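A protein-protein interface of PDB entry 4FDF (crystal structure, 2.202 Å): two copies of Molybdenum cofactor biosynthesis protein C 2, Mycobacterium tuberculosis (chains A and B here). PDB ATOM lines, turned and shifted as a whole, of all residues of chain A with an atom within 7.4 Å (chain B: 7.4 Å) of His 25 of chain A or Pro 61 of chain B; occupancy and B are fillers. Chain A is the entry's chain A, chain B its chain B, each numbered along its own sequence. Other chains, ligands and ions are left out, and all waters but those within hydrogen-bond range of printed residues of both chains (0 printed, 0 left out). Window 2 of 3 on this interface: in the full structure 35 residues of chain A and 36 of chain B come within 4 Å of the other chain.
O of Ala 23 of chain A is in hydrogen-bond range of N of Asp 64 of chain B (2.6 Å). The backbone carbonyl oxygen (O) of Pro 61 of chain B is in hydrogen-bond range of a ring nitrogen (NE2) of His 25 of chain A. The backbone carbonyl oxygen (O) of Lys 62 of chain B lies within hydrogen-bond range of the backbone NH (N) of His 25 of chain A (3.2 Å).
Of chain B, only Pro 61 (2.8 Å) and Lys 62 (3.2 Å) come within 4 Å of His 25 of chain A. Of the printed residues of chain B, Leu 86 of chain A touches Lys 62 (3.7 Å) and Met 138 (3.4 Å). Leu 54 of chain B touches none of the printed residues of chain A. Gly 59 of chain B touches none of the printed residues of chain A. Pro 61 of chain B touches just one residue of chain A: His 25. Printed residues of chain A within 4 Å of Gly 63 of chain B: Ala 23. The nearest residue of chain A that does not touch Pro 61 of chain B is Ala 24 of chain A (6.5 Å).
OG1 of Thr 68 of chain B is in hydrogen-bond range of O of Asp 64 of chain B, at 2.9 Å.
Of the 13 printed residues of chain B, 6 touch a printed residue of chain A. Hydrophobic or aromatic side chains of chain B that line the printed part of chain A: Met 138. Of the 7 printed residues of chain A, 4 touch a printed residue of chain B. Among the printed residues, 8 pairs touch across the chains. Among the printed residues, no Asp or Glu carboxylate lies within 4 Å of a Lys or Arg side-chain nitrogen of the other chain.
Gly 63 of chain B touches Ala 23 of chain A. Ala 24 of chain A touches Lys 62 of chain B. OG1 of Thr 68 of chain B touches CB of Ala 24 of chain A, 3.8 Å away. Leu 86 of chain A touches Lys 62 of chain B. Met 138 of chain B touches Leu 86 of chain A.
No position is printed for both chains. Of the 8 pairs that touch across the chains among the printed residues, none has its exchanged pair printed and touching as well.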
ATOM      1  N   ALA A  23      25.759  12.170  22.311  1.00  0.00           N
ATOM      2  CA  ALA A  23      27.120  11.951  21.820  1.00  0.00           C
ATOM      3  C   ALA A  23      27.359  12.118  20.324  1.00  0.00           C
ATOM      4  O   ALA A  23      26.949  13.109  19.731  1.00  0.00           O
ATOM      5  N   ALA A  24      28.033  11.139  19.719  1.00  0.00           N
ATOM      6  CA  ALA A  24      28.597  11.279  18.368  1.00  0.00           C
ATOM      7  C   ALA A  24      29.004   9.937  17.745  1.00  0.00           C
ATOM      8  O   ALA A  24      28.968   8.894  18.404  1.00  0.00           O
ATOM      9  CB  ALA A  24      29.806  12.234  18.402  1.00  0.00           C
ATOM     10  N   HIS A  25      29.380   9.987  16.467  1.00  0.00           N
ATOM     11  CA  HIS A  25      29.955   8.854  15.728  1.00  0.00           C
ATOM     12  C   HIS A  25      30.324   9.301  14.337  1.00  0.00           C
ATOM     13  O   HIS A  25      29.556  10.019  13.684  1.00  0.00           O
ATOM     14  CB  HIS A  25      28.995   7.661  15.671  1.00  0.00           C
ATOM     15  CG  HIS A  25      27.890   7.809  14.650  1.00  0.00           C
ATOM     16  ND1 HIS A  25      27.926   7.196  13.451  1.00  0.00           N
ATOM     17  CD2 HIS A  25      26.704   8.541  14.683  1.00  0.00           C
ATOM     18  CE1 HIS A  25      26.820   7.513  12.751  1.00  0.00           C
ATOM     19  NE2 HIS A  25      26.072   8.337  13.507  1.00  0.00           N
ATOM     20  N   MET A  26      31.503   8.899  13.870  1.00  0.00           N
ATOM     21  CA  MET A  26      31.915   9.245  12.510  1.00  0.00           C
ATOM     22  C   MET A  26      31.372   8.253  11.473  1.00  0.00           C
ATOM     23  O   MET A  26      30.870   7.183  11.831  1.00  0.00           O
ATOM     24  CB  MET A  26      33.441   9.432  12.399  1.00  0.00           C
ATOM     25  CG  MET A  26      34.323   8.261  12.824  1.00  0.00           C
ATOM     26  SD  MET A  26      36.066   8.527  12.362  1.00  0.00           S
ATOM     27  CE  MET A  26      36.526   9.920  13.399  1.00  0.00           C
ATOM     28  N   VAL A  27      31.454   8.634  10.198  1.00  0.00           N
ATOM     29  CA  VAL A  27      31.072   7.763   9.084  1.00  0.00           C
ATOM     30  C   VAL A  27      32.128   6.711   8.782  1.00  0.00           C
ATOM     31  O   VAL A  27      33.224   6.747   9.347  1.00  0.00           O
ATOM     32  N   ASP A  28      31.803   5.793   7.867  1.00  0.00           N
ATOM     33  CA  ASP A  28      32.637   4.618   7.567  1.00  0.00           C
ATOM     34  C   ASP A  28      33.356   4.672   6.211  1.00  0.00           C
ATOM     35  O   ASP A  28      33.332   5.702   5.531  1.00  0.00           O
ATOM     36  CB  ASP A  28      31.762   3.366   7.615  1.00  0.00           C
ATOM     37  CG  ASP A  28      32.369   2.270   8.452  1.00  0.00           C
ATOM     38  OD1 ASP A  28      31.706   1.872   9.426  1.00  0.00           O
ATOM     39  OD2 ASP A  28      33.499   1.823   8.155  1.00  0.00           O
ATOM     40  N   LEU A  86      35.251  14.555  14.556  1.00  0.00           N
ATOM     41  CA  LEU A  86      34.676  13.490  13.739  1.00  0.00           C
ATOM     42  C   LEU A  86      35.217  13.390  12.309  1.00  0.00           C
ATOM     43  O   LEU A  86      34.710  12.605  11.509  1.00  0.00           O
ATOM     44  CB  LEU A  86      33.139  13.538  13.762  1.00  0.00           C
ATOM     45  CG  LEU A  86      32.460  13.257  15.110  1.00  0.00           C
ATOM     46  CD1 LEU A  86      30.975  12.927  14.906  1.00  0.00           C
ATOM     47  CD2 LEU A  86      33.132  12.114  15.863  1.00  0.00           C
ATOM     48  N   LEU B  54      16.688  19.715  13.490  1.00  0.00           N
ATOM     49  CA  LEU B  54      17.395  18.481  13.831  1.00  0.00           C
ATOM     50  C   LEU B  54      18.268  18.607  15.080  1.00  0.00           C
ATOM     51  O   LEU B  54      18.516  17.614  15.774  1.00  0.00           O
ATOM     52  CB  LEU B  54      18.200  17.961  12.639  1.00  0.00           C
ATOM     53  CG  LEU B  54      17.415  17.603  11.367  1.00  0.00           C
ATOM     54  CD1 LEU B  54      18.374  17.232  10.241  1.00  0.00           C
ATOM     55  CD2 LEU B  54      16.388  16.483  11.597  1.00  0.00           C
ATOM     56  N   GLY B  58      17.539  16.544  18.462  1.00  0.00           N
ATOM     57  CA  GLY B  58      18.663  15.617  18.607  1.00  0.00           C
ATOM     58  C   GLY B  58      18.755  14.636  17.451  1.00  0.00           C
ATOM     59  O   GLY B  58      19.260  13.524  17.619  1.00  0.00           O
ATOM     60  N   GLY B  59      18.286  15.054  16.274  1.00  0.00           N
ATOM     61  CA  GLY B  59      18.154  14.156  15.133  1.00  0.00           C
ATOM     62  C   GLY B  59      19.224  14.223  14.058  1.00  0.00           C
ATOM     63  O   GLY B  59      19.047  13.644  12.989  1.00  0.00           O
ATOM     64  N   LEU B  60      20.329  14.918  14.322  1.00  0.00           N
ATOM     65  CA  LEU B  60      21.437  14.974  13.364  1.00  0.00           C
ATOM     66  C   LEU B  60      22.075  13.603  13.190  1.00  0.00           C
ATOM     67  O   LEU B  60      22.285  12.888  14.178  1.00  0.00           O
ATOM     68  CB  LEU B  60      22.514  15.963  13.810  1.00  0.00           C
ATOM     69  CG  LEU B  60      22.199  17.448  13.713  1.00  0.00           C
ATOM     70  CD1 LEU B  60      23.326  18.240  14.370  1.00  0.00           C
ATOM     71  CD2 LEU B  60      22.007  17.858  12.256  1.00  0.00           C
ATOM     72  N   PRO B  61      22.398  13.232  11.937  1.00  0.00           N
ATOM     73  CA  PRO B  61      23.009  11.926  11.695  1.00  0.00           C
ATOM     74  C   PRO B  61      24.283  11.700  12.516  1.00  0.00           C
ATOM     75  O   PRO B  61      24.484  10.616  13.068  1.00  0.00           O
ATOM     76  CB  PRO B  61      23.326  11.961  10.195  1.00  0.00           C
ATOM     77  CG  PRO B  61      22.315  12.906   9.631  1.00  0.00           C
ATOM     78  CD  PRO B  61      22.163  13.970  10.683  1.00  0.00           C
ATOM     79  N   LYS B  62      25.118  12.724  12.626  1.00  0.00           N
ATOM     80  CA  LYS B  62      26.440  12.542  13.213  1.00  0.00           C
ATOM     81  C   LYS B  62      26.440  12.629  14.749  1.00  0.00           C
ATOM     82  O   LYS B  62      27.406  12.232  15.396  1.00  0.00           O
ATOM     83  CB  LYS B  62      27.418  13.531  12.584  1.00  0.00           C
ATOM     84  CG  LYS B  62      28.636  12.877  11.969  1.00  0.00           C
ATOM     85  CD  LYS B  62      29.122  13.694  10.791  1.00  0.00           C
ATOM     86  CE  LYS B  62      30.634  13.716  10.710  1.00  0.00           C
ATOM     87  NZ  LYS B  62      31.066  14.612   9.602  1.00  0.00           N
ATOM     88  N   GLY B  63      25.350  13.135  15.320  1.00  0.00           N
ATOM     89  CA  GLY B  63      25.179  13.168  16.770  1.00  0.00           C
ATOM     90  C   GLY B  63      24.979  14.565  17.322  1.00  0.00           C
ATOM     91  O   GLY B  63      24.490  15.453  16.623  1.00  0.00           O
ATOM     92  N   ASP B  64      25.353  14.751  18.587  1.00  0.00           N
ATOM     93  CA  ASP B  64      25.176  16.017  19.297  1.00  0.00           C
ATOM     94  C   ASP B  64      26.195  17.052  18.812  1.00  0.00           C
ATOM     95  O   ASP B  64      27.331  17.089  19.296  1.00  0.00           O
ATOM     96  CB  ASP B  64      25.295  15.787  20.813  1.00  0.00           C
ATOM     97  CG  ASP B  64      24.901  17.019  21.642  1.00  0.00           C
ATOM     98  OD1 ASP B  64      24.871  18.150  21.105  1.00  0.00           O
ATOM     99  OD2 ASP B  64      24.620  16.852  22.847  1.00  0.00           O
ATOM    100  N   THR B  68      29.744  18.359  20.845  1.00  0.00           N
ATOM    101  CA  THR B  68      30.958  18.034  20.103  1.00  0.00           C
ATOM    102  C   THR B  68      31.760  19.309  19.802  1.00  0.00           C
ATOM    103  O   THR B  68      32.978  19.338  19.979  1.00  0.00           O
ATOM    104  CB  THR B  68      30.653  17.206  18.821  1.00  0.00           C
ATOM    105  OG1 THR B  68      30.016  15.978  19.195  1.00  0.00           O
ATOM    106  CG2 THR B  68      31.928  16.865  18.039  1.00  0.00           C
ATOM    107  N   MET B 138      29.283  18.724  11.553  1.00  0.00           N
ATOM    108  CA  MET B 138      28.149  17.971  12.052  1.00  0.00           C
ATOM    109  C   MET B 138      26.904  18.159  11.185  1.00  0.00           C
ATOM    110  O   MET B 138      26.013  17.307  11.189  1.00  0.00           O
ATOM    111  CB  MET B 138      27.833  18.361  13.505  1.00  0.00           C
ATOM    112  CG  MET B 138      28.987  18.205  14.491  1.00  0.00           C
ATOM    113  SD  MET B 138      29.376  16.513  14.981  1.00  0.00           S
ATOM    114  CE  MET B 138      30.254  15.966  13.548  1.00  0.00           C
ATOM    115  N   ILE B 139      26.838  19.272  10.456  1.00  0.00           N
ATOM    116  CA  ILE B 139      25.612  19.628   9.739  1.00  0.00           C
ATOM    117  C   ILE B 139      25.742  19.616   8.214  1.00  0.00           C
ATOM    118  O   ILE B 139      24.736  19.731   7.517  1.00  0.00           O
ATOM    119  CB  ILE B 139      24.992  20.987  10.243  1.00  0.00           C
ATOM    120  CG1 ILE B 139      25.795  22.201   9.760  1.00  0.00           C
ATOM    121  CG2 ILE B 139      24.848  21.005  11.763  1.00  0.00           C
ATOM    122  CD1 ILE B 139      25.184  22.889   8.564  1.00  0.00           C
ATOM    123  N   ALA B 141      25.993  17.540   5.919  1.00  0.00           N
ATOM    124  CA  ALA B 141      25.239  16.536   5.162  1.00  0.00           C
ATOM    125  C   ALA B 141      23.768  16.936   4.955  1.00  0.00           C
ATOM    126  O   ALA B 141      23.137  16.509   3.987  1.00  0.00           O
ATOM    127  CB  ALA B 141      25.342  15.164   5.832  1.00  0.00           C
ATOM    128  N   VAL B 142      23.238  17.748   5.874  1.00  0.00           N
ATOM    129  CA  VAL B 142      21.888  18.309   5.765  1.00  0.00           C
ATOM    130  C   VAL B 142      21.905  19.666   5.055  1.00  0.00           C
ATOM    131  O   VAL B 142      21.017  19.963   4.256  1.00  0.00           O
ATOM    132  CB  VAL B 142      21.215  18.461   7.158  1.00  0.00           C
ATOM    133  CG1 VAL B 142      19.780  18.956   7.024  1.00  0.00           C
ATOM    134  CG2 VAL B 142      21.255  17.153   7.930  1.00  0.00           C
